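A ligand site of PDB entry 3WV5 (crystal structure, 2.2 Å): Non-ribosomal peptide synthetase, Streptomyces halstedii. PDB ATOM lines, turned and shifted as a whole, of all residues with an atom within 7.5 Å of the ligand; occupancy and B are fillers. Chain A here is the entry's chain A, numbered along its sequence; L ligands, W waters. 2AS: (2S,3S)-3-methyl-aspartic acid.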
ATOM      1  N   THR A 201       1.797  16.636 -10.426  1.00  0.00           N
ATOM      2  CA  THR A 201       1.360  15.231 -10.657  1.00  0.00           C
ATOM      3  C   THR A 201       1.573  14.749 -12.104  1.00  0.00           C
ATOM      4  O   THR A 201       1.402  13.576 -12.428  1.00  0.00           O
ATOM      5  CB  THR A 201      -0.160  15.121 -10.431  1.00  0.00           C
ATOM      6  OG1 THR A 201      -0.832  16.066 -11.296  1.00  0.00           O
ATOM      7  CG2 THR A 201      -0.516  15.416  -8.958  1.00  0.00           C
ATOM      8  N   ILE A 225      -7.539  12.760   8.090  1.00  0.00           N
ATOM      9  CA  ILE A 225      -6.868  11.463   7.935  1.00  0.00           C
ATOM     10  C   ILE A 225      -6.534  10.894   9.302  1.00  0.00           C
ATOM     11  O   ILE A 225      -6.772   9.706   9.594  1.00  0.00           O
ATOM     12  CB  ILE A 225      -5.580  11.563   7.082  1.00  0.00           C
ATOM     13  CG1 ILE A 225      -5.994  11.824   5.643  1.00  0.00           C
ATOM     14  CG2 ILE A 225      -4.748  10.276   7.167  1.00  0.00           C
ATOM     15  CD1 ILE A 225      -4.902  12.449   4.795  1.00  0.00           C
ATOM     16  N   TRP A 245       5.745  13.856  -3.348  1.00  0.00           N
ATOM     17  CA  TRP A 245       4.448  13.187  -3.523  1.00  0.00           C
ATOM     18  C   TRP A 245       3.641  13.554  -2.239  1.00  0.00           C
ATOM     19  O   TRP A 245       4.236  13.583  -1.166  1.00  0.00           O
ATOM     20  CB  TRP A 245       4.747  11.675  -3.559  1.00  0.00           C
ATOM     21  CG  TRP A 245       3.683  10.711  -3.929  1.00  0.00           C
ATOM     22  CD1 TRP A 245       2.352  10.923  -4.189  1.00  0.00           C
ATOM     23  CD2 TRP A 245       3.864   9.299  -3.983  1.00  0.00           C
ATOM     24  NE1 TRP A 245       1.698   9.715  -4.462  1.00  0.00           N
ATOM     25  CE2 TRP A 245       2.617   8.717  -4.336  1.00  0.00           C
ATOM     26  CE3 TRP A 245       4.971   8.477  -3.779  1.00  0.00           C
ATOM     27  CZ2 TRP A 245       2.469   7.372  -4.505  1.00  0.00           C
ATOM     28  CZ3 TRP A 245       4.829   7.128  -3.960  1.00  0.00           C
ATOM     29  CH2 TRP A 245       3.579   6.579  -4.308  1.00  0.00           C
ATOM     30  N   ASP A 246       2.330  13.811  -2.341  1.00  0.00           N
ATOM     31  CA  ASP A 246       1.588  14.108  -1.111  1.00  0.00           C
ATOM     32  C   ASP A 246       1.559  12.932  -0.106  1.00  0.00           C
ATOM     33  O   ASP A 246       1.283  13.126   1.095  1.00  0.00           O
ATOM     34  CB  ASP A 246       0.171  14.672  -1.396  1.00  0.00           C
ATOM     35  CG  ASP A 246      -0.859  13.616  -1.838  1.00  0.00           C
ATOM     36  OD1 ASP A 246      -0.655  12.399  -1.710  1.00  0.00           O
ATOM     37  OD2 ASP A 246      -1.914  14.062  -2.348  1.00  0.00           O
ATOM     38  N   PHE A 247       1.935  11.735  -0.572  1.00  0.00           N
ATOM     39  CA  PHE A 247       2.052  10.605   0.336  1.00  0.00           C
ATOM     40  C   PHE A 247       3.106  10.879   1.368  1.00  0.00           C
ATOM     41  O   PHE A 247       2.808  10.818   2.574  1.00  0.00           O
ATOM     42  CB  PHE A 247       2.347   9.286  -0.423  1.00  0.00           C
ATOM     43  CG  PHE A 247       1.587   8.107   0.091  1.00  0.00           C
ATOM     44  CD1 PHE A 247       1.224   7.988   1.419  1.00  0.00           C
ATOM     45  CD2 PHE A 247       1.228   7.097  -0.760  1.00  0.00           C
ATOM     46  CE1 PHE A 247       0.523   6.900   1.903  1.00  0.00           C
ATOM     47  CE2 PHE A 247       0.538   5.965  -0.283  1.00  0.00           C
ATOM     48  CZ  PHE A 247       0.187   5.864   1.038  1.00  0.00           C
ATOM     49  N   GLY A 248       4.299  11.276   0.952  1.00  0.00           N
ATOM     50  CA  GLY A 248       5.315  11.648   1.947  1.00  0.00           C
ATOM     51  C   GLY A 248       5.101  12.998   2.646  1.00  0.00           C
ATOM     52  O   GLY A 248       5.395  13.173   3.828  1.00  0.00           O
ATOM     53  N   TYR A 250       2.531  14.294   3.609  1.00  0.00           N
ATOM     54  CA  TYR A 250       1.532  14.199   4.731  1.00  0.00           C
ATOM     55  C   TYR A 250       1.966  13.334   5.889  1.00  0.00           C
ATOM     56  O   TYR A 250       1.368  13.416   6.964  1.00  0.00           O
ATOM     57  CB  TYR A 250       0.215  13.785   4.186  1.00  0.00           C
ATOM     58  CG  TYR A 250      -0.596  14.949   3.671  1.00  0.00           C
ATOM     59  CD1 TYR A 250      -1.696  15.425   4.370  1.00  0.00           C
ATOM     60  CD2 TYR A 250      -0.269  15.550   2.490  1.00  0.00           C
ATOM     61  CE1 TYR A 250      -2.471  16.471   3.896  1.00  0.00           C
ATOM     62  CE2 TYR A 250      -1.037  16.578   1.984  1.00  0.00           C
ATOM     63  CZ  TYR A 250      -2.118  17.075   2.694  1.00  0.00           C
ATOM     64  OH  TYR A 250      -2.825  18.176   2.172  1.00  0.00           O
ATOM     65  N   LYS A 251       2.994  12.498   5.691  1.00  0.00           N
ATOM     66  CA  LYS A 251       3.634  11.823   6.819  1.00  0.00           C
ATOM     67  C   LYS A 251       4.484  12.894   7.599  1.00  0.00           C
ATOM     68  O   LYS A 251       4.508  12.873   8.847  1.00  0.00           O
ATOM     69  CB  LYS A 251       4.333  10.512   6.350  1.00  0.00           C
ATOM     70  CG  LYS A 251       3.285   9.313   6.085  1.00  0.00           C
ATOM     71  CD  LYS A 251       1.673   9.564   6.231  1.00  0.00           C
ATOM     72  CE  LYS A 251       0.981   9.884   4.888  1.00  0.00           C
ATOM     73  NZ  LYS A 251      -0.486   9.649   4.561  1.00  0.00           N
ATOM     74  N   ILE A 287       2.360   2.519   2.624  1.00  0.00           N
ATOM     75  CA  ILE A 287       2.738   1.624   1.641  1.00  0.00           C
ATOM     76  C   ILE A 287       1.998   1.927   0.385  1.00  0.00           C
ATOM     77  O   ILE A 287       0.902   2.565   0.366  1.00  0.00           O
ATOM     78  CB  ILE A 287       2.473   0.118   2.018  1.00  0.00           C
ATOM     79  CG1 ILE A 287       1.039  -0.073   2.466  1.00  0.00           C
ATOM     80  CG2 ILE A 287       3.449  -0.338   3.072  1.00  0.00           C
ATOM     81  CD1 ILE A 287       0.657  -1.577   2.538  1.00  0.00           C
ATOM     82  N   VAL A 288       2.567   1.353  -0.647  1.00  0.00           N
ATOM     83  CA  VAL A 288       1.910   1.204  -1.955  1.00  0.00           C
ATOM     84  C   VAL A 288       2.006  -0.281  -2.310  1.00  0.00           C
ATOM     85  O   VAL A 288       2.808  -0.983  -1.718  1.00  0.00           O
ATOM     86  CB  VAL A 288       2.712   2.236  -2.859  1.00  0.00           C
ATOM     87  CG1 VAL A 288       3.228   1.613  -4.079  1.00  0.00           C
ATOM     88  CG2 VAL A 288       1.952   3.535  -3.083  1.00  0.00           C
ATOM     89  N   ASN A 314      -2.247   1.848   2.938  1.00  0.00           N
ATOM     90  CA  ASN A 314      -2.075   1.738   1.521  1.00  0.00           C
ATOM     91  C   ASN A 314      -2.969   2.721   0.768  1.00  0.00           C
ATOM     92  O   ASN A 314      -4.167   2.882   1.099  1.00  0.00           O
ATOM     93  CB  ASN A 314      -2.338   0.318   1.030  1.00  0.00           C
ATOM     94  CG  ASN A 314      -2.087   0.174  -0.454  1.00  0.00           C
ATOM     95  OD1 ASN A 314      -0.961  -0.048  -0.899  1.00  0.00           O
ATOM     96  ND2 ASN A 314      -3.155   0.353  -1.233  1.00  0.00           N
ATOM     97  N   SER A 315      -2.353   3.436  -0.199  1.00  0.00           N
ATOM     98  CA  SER A 315      -3.116   4.182  -1.163  1.00  0.00           C
ATOM     99  C   SER A 315      -2.418   4.100  -2.504  1.00  0.00           C
ATOM    100  O   SER A 315      -1.503   3.336  -2.663  1.00  0.00           O
ATOM    101  CB  SER A 315      -3.277   5.665  -0.750  1.00  0.00           C
ATOM    102  OG  SER A 315      -4.438   6.207  -1.335  1.00  0.00           O
ATOM    103  N   ALA A 316      -2.895   4.915  -3.451  1.00  0.00           N
ATOM    104  CA  ALA A 316      -2.281   5.068  -4.752  1.00  0.00           C
ATOM    105  C   ALA A 316      -2.713   3.978  -5.711  1.00  0.00           C
ATOM    106  O   ALA A 316      -2.900   4.293  -6.867  1.00  0.00           O
ATOM    107  CB  ALA A 316      -0.784   5.145  -4.689  1.00  0.00           C
ATOM    108  N   ALA A 317      -2.894   2.730  -5.255  1.00  0.00           N
ATOM    109  CA  ALA A 317      -3.295   1.647  -6.129  1.00  0.00           C
ATOM    110  C   ALA A 317      -3.877   0.548  -5.330  1.00  0.00           C
ATOM    111  O   ALA A 317      -3.703   0.474  -4.119  1.00  0.00           O
ATOM    112  CB  ALA A 317      -2.106   1.109  -6.971  1.00  0.00           C
ATOM    113  N   MET A 339      -6.965   2.684   1.615  1.00  0.00           N
ATOM    114  CA  MET A 339      -7.323   4.044   1.376  1.00  0.00           C
ATOM    115  C   MET A 339      -7.359   4.279  -0.105  1.00  0.00           C
ATOM    116  O   MET A 339      -6.888   3.444  -0.884  1.00  0.00           O
ATOM    117  CB  MET A 339      -6.309   5.002   2.007  1.00  0.00           C
ATOM    118  CG  MET A 339      -5.887   4.540   3.385  1.00  0.00           C
ATOM    119  SD  MET A 339      -4.876   5.633   4.371  1.00  0.00           S
ATOM    120  CE  MET A 339      -3.394   5.736   3.301  1.00  0.00           C
ATOM    121  N   TYR A 340      -7.940   5.400  -0.494  1.00  0.00           N
ATOM    122  CA  TYR A 340      -8.006   5.824  -1.881  1.00  0.00           C
ATOM    123  C   TYR A 340      -7.999   7.343  -1.866  1.00  0.00           C
ATOM    124  O   TYR A 340      -8.645   7.974  -1.023  1.00  0.00           O
ATOM    125  CB  TYR A 340      -9.300   5.279  -2.539  1.00  0.00           C
ATOM    126  CG  TYR A 340      -9.863   6.090  -3.670  1.00  0.00           C
ATOM    127  CD1 TYR A 340      -9.159   6.264  -4.846  1.00  0.00           C
ATOM    128  CD2 TYR A 340     -11.153   6.646  -3.587  1.00  0.00           C
ATOM    129  CE1 TYR A 340      -9.695   6.983  -5.914  1.00  0.00           C
ATOM    130  CE2 TYR A 340     -11.714   7.373  -4.637  1.00  0.00           C
ATOM    131  CZ  TYR A 340     -10.975   7.535  -5.802  1.00  0.00           C
ATOM    132  OH  TYR A 340     -11.500   8.270  -6.845  1.00  0.00           O
ATOM    133  N   GLY A 341      -7.286   7.943  -2.803  1.00  0.00           N
ATOM    134  CA  GLY A 341      -7.258   9.385  -2.934  1.00  0.00           C
ATOM    135  C   GLY A 341      -6.774   9.894  -4.266  1.00  0.00           C
ATOM    136  O   GLY A 341      -6.298   9.131  -5.127  1.00  0.00           O
ATOM    137  N   GLN A 342      -6.907  11.201  -4.418  1.00  0.00           N
ATOM    138  CA  GLN A 342      -6.262  11.964  -5.480  1.00  0.00           C
ATOM    139  C   GLN A 342      -5.635  13.158  -4.878  1.00  0.00           C
ATOM    140  O   GLN A 342      -6.197  13.746  -3.960  1.00  0.00           O
ATOM    141  CB  GLN A 342      -7.305  12.464  -6.506  1.00  0.00           C
ATOM    142  CG  GLN A 342      -7.955  11.353  -7.247  1.00  0.00           C
ATOM    143  CD  GLN A 342      -8.798  11.876  -8.354  1.00  0.00           C
ATOM    144  OE1 GLN A 342      -9.255  13.017  -8.338  1.00  0.00           O
ATOM    145  NE2 GLN A 342      -9.024  11.038  -9.344  1.00  0.00           N
ATOM    146  N   THR A 343      -4.553  13.632  -5.496  1.00  0.00           N
ATOM    147  CA  THR A 343      -3.840  14.784  -4.995  1.00  0.00           C
ATOM    148  C   THR A 343      -4.792  15.989  -4.952  1.00  0.00           C
ATOM    149  O   THR A 343      -4.747  16.806  -4.041  1.00  0.00           O
ATOM    150  CB  THR A 343      -2.581  15.040  -5.856  1.00  0.00           C
ATOM    151  OG1 THR A 343      -1.694  13.940  -5.741  1.00  0.00           O
ATOM    152  CG2 THR A 343      -1.857  16.296  -5.347  1.00  0.00           C
ATOM    153  N   GLU A 344      -5.680  16.072  -5.934  1.00  0.00           N
ATOM    154  CA  GLU A 344      -6.737  17.114  -6.016  1.00  0.00           C
ATOM    155  C   GLU A 344      -7.481  17.413  -4.732  1.00  0.00           C
ATOM    156  O   GLU A 344      -7.928  18.554  -4.533  1.00  0.00           O
ATOM    157  CB  GLU A 344      -7.759  16.688  -7.064  1.00  0.00           C
ATOM    158  CG  GLU A 344      -7.332  16.934  -8.486  1.00  0.00           C
ATOM    159  CD  GLU A 344      -6.321  15.932  -9.048  1.00  0.00           C
ATOM    160  OE1 GLU A 344      -5.846  14.998  -8.350  1.00  0.00           O
ATOM    161  OE2 GLU A 344      -5.967  16.101 -10.209  1.00  0.00           O
ATOM    162  N   CYS A 345      -7.651  16.408  -3.848  1.00  0.00           N
ATOM    163  CA  CYS A 345      -8.184  16.672  -2.496  1.00  0.00           C
ATOM    164  C   CYS A 345      -7.432  15.916  -1.406  1.00  0.00           C
ATOM    165  O   CYS A 345      -7.991  15.630  -0.340  1.00  0.00           O
ATOM    166  CB  CYS A 345      -9.646  16.283  -2.424  1.00  0.00           C
ATOM    167  SG  CYS A 345     -10.009  14.565  -2.774  1.00  0.00           S
ATOM    168  N   LYS A 346      -6.156  15.629  -1.666  1.00  0.00           N
ATOM    169  CA  LYS A 346      -5.271  14.766  -0.846  1.00  0.00           C
ATOM    170  C   LYS A 346      -5.762  13.314  -0.775  1.00  0.00           C
ATOM    171  O   LYS A 346      -5.107  12.435  -1.311  1.00  0.00           O
ATOM    172  CB  LYS A 346      -5.025  15.300   0.567  1.00  0.00           C
ATOM    173  CG  LYS A 346      -4.404  14.247   1.526  1.00  0.00           C
ATOM    174  CD  LYS A 346      -3.115  13.609   0.960  1.00  0.00           C
ATOM    175  CE  LYS A 346      -2.569  12.538   1.897  1.00  0.00           C
ATOM    176  NZ  LYS A 346      -1.265  12.035   1.429  1.00  0.00           N
ATOM    177  N   ARG A 347      -6.926  13.096  -0.153  1.00  0.00           N
ATOM    178  CA  ARG A 347      -7.438  11.758   0.046  1.00  0.00           C
ATOM    179  C   ARG A 347      -8.934  11.760   0.098  1.00  0.00           C
ATOM    180  O   ARG A 347      -9.548  12.753   0.477  1.00  0.00           O
ATOM    181  CB  ARG A 347      -6.813  11.133   1.290  1.00  0.00           C
ATOM    182  CG  ARG A 347      -7.195   9.683   1.548  1.00  0.00           C
ATOM    183  CD  ARG A 347      -6.263   8.996   2.566  1.00  0.00           C
ATOM    184  NE  ARG A 347      -4.936   8.923   2.004  1.00  0.00           N
ATOM    185  CZ  ARG A 347      -3.809   8.936   2.701  1.00  0.00           C
ATOM    186  NH1 ARG A 347      -3.817   8.953   4.052  1.00  0.00           N
ATOM    187  NH2 ARG A 347      -2.645   8.873   2.070  1.00  0.00           N
ATOM    188  N   ILE A 348      -9.532  10.618  -0.264  1.00  0.00           N
ATOM    189  CA  ILE A 348     -10.953  10.555  -0.457  1.00  0.00           C
ATOM    190  C   ILE A 348     -11.676   9.627   0.527  1.00  0.00           C
ATOM    191  O   ILE A 348     -12.675  10.043   1.145  1.00  0.00           O
ATOM    192  CB  ILE A 348     -11.250  10.145  -1.896  1.00  0.00           C
ATOM    193  CG1 ILE A 348     -10.916  11.300  -2.818  1.00  0.00           C
ATOM    194  CG2 ILE A 348     -12.714   9.808  -2.040  1.00  0.00           C
ATOM    195  CD1 ILE A 348     -10.875  10.912  -4.283  1.00  0.00           C
ATOM    196  N   SER A 349     -11.180   8.429   0.680  1.00  0.00           N
ATOM    197  CA  SER A 349     -11.743   7.468   1.587  1.00  0.00           C
ATOM    198  C   SER A 349     -10.614   6.763   2.348  1.00  0.00           C
ATOM    199  O   SER A 349      -9.528   6.536   1.822  1.00  0.00           O
ATOM    200  CB  SER A 349     -12.602   6.434   0.825  1.00  0.00           C
ATOM    201  OG  SER A 349     -11.801   5.650  -0.081  1.00  0.00           O
ATOM    202  N   ILE A 350     -10.946   6.358   3.568  1.00  0.00           N
ATOM    203  CA  ILE A 350     -10.178   5.435   4.391  1.00  0.00           C
ATOM    204  C   ILE A 350     -11.124   4.361   4.966  1.00  0.00           C
ATOM    205  O   ILE A 350     -12.227   4.672   5.493  1.00  0.00           O
ATOM    206  CB  ILE A 350      -9.473   6.163   5.545  1.00  0.00           C
ATOM    207  CG1 ILE A 350      -8.444   7.173   4.995  1.00  0.00           C
ATOM    208  CG2 ILE A 350      -8.742   5.172   6.418  1.00  0.00           C
ATOM    209  CD1 ILE A 350      -7.893   8.094   6.072  1.00  0.00           C
HETATM  210  C   2AS L   1      -3.680   9.735  -1.112  1.00  0.00           C
HETATM  211  O   2AS L   1      -2.910  10.211  -0.259  1.00  0.00           O
HETATM  212  CA  2AS L   1      -3.608  10.118  -2.576  1.00  0.00           C
HETATM  213  N   2AS L   1      -2.965  11.467  -2.806  1.00  0.00           N
HETATM  214  CB  2AS L   1      -2.823   9.054  -3.322  1.00  0.00           C
HETATM  215  CG  2AS L   1      -2.670   9.368  -4.827  1.00  0.00           C
HETATM  216  OD1 2AS L   1      -2.173   8.503  -5.545  1.00  0.00           O
HETATM  217  C4  2AS L   1      -1.466   8.960  -2.682  1.00  0.00           C
HETATM  218  OD2 2AS L   1      -3.024  10.441  -5.370  1.00  0.00           O
HETATM  219  OXT 2AS L   1      -4.492   8.859  -0.779  1.00  0.00           O
HETATM  220  O   HOH W   1       0.153   8.978  -7.459  1.00  0.00           O
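Residues that only touch the ligand: Trp 245, Phe 247, Ala 316, Tyr 340, Gly 341, Gln 342 and Thr 343. 11 residues have an atom within 4 Å of the ligand: Trp 245, Asp 246, Phe 247, Ser 315, Ala 316, Tyr 340, Gly 341, Gln 342, Thr 343, Lys 346 and Arg 347. The nearest printed residue that does not touch the ligand is Met 339 (5.1 Å).
The side-chain sulfur of Met 339 sits close to the guanidinium group of Arg 347, at 3.5 Å. O of Arg 347 sits at hydrogen-bond distance from SG of Cys 345 (3.8 Å). The backbone carbonyl oxygen (O) of Ile 287 is in hydrogen-bond range of the backbone NH (N) of Ser 315 (3.4 Å). NZ of Lys 346 lies within salt-bridge range of OD1 of Asp 246 (3.2 Å). OG1 of Thr 343 lies close to OD2 of Asp 246, at 3.4 Å. O of Tyr 340 is in hydrogen-bond range of N of Ile 348 (2.9 Å). The backbone carbonyl oxygen of Ser 349 lies within hydrogen-bond range of the backbone NH of Tyr 340.
Water W1 bridges OD1 of the ligand (3.0 Å) and NE1 of Trp 245 (3.5 Å).
The guanidinium group (NH2) of Arg 347 is in salt-bridge range of an oxygen (O) of the ligand (2.7 Å). OXT of the ligand lies within hydrogen-bond range of OG of Ser 315, 2.7 Å away. A nitrogen (N) of the ligand is in salt-bridge range of the side-chain carboxylate (OD1) of Asp 246 (2.7 Å). A nitrogen (N) of the ligand lies within hydrogen-bond range of the backbone carbonyl oxygen (O) of Lys 346. An oxygen (O) of the ligand is in salt-bridge range of the side-chain amino group of Lys 346.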
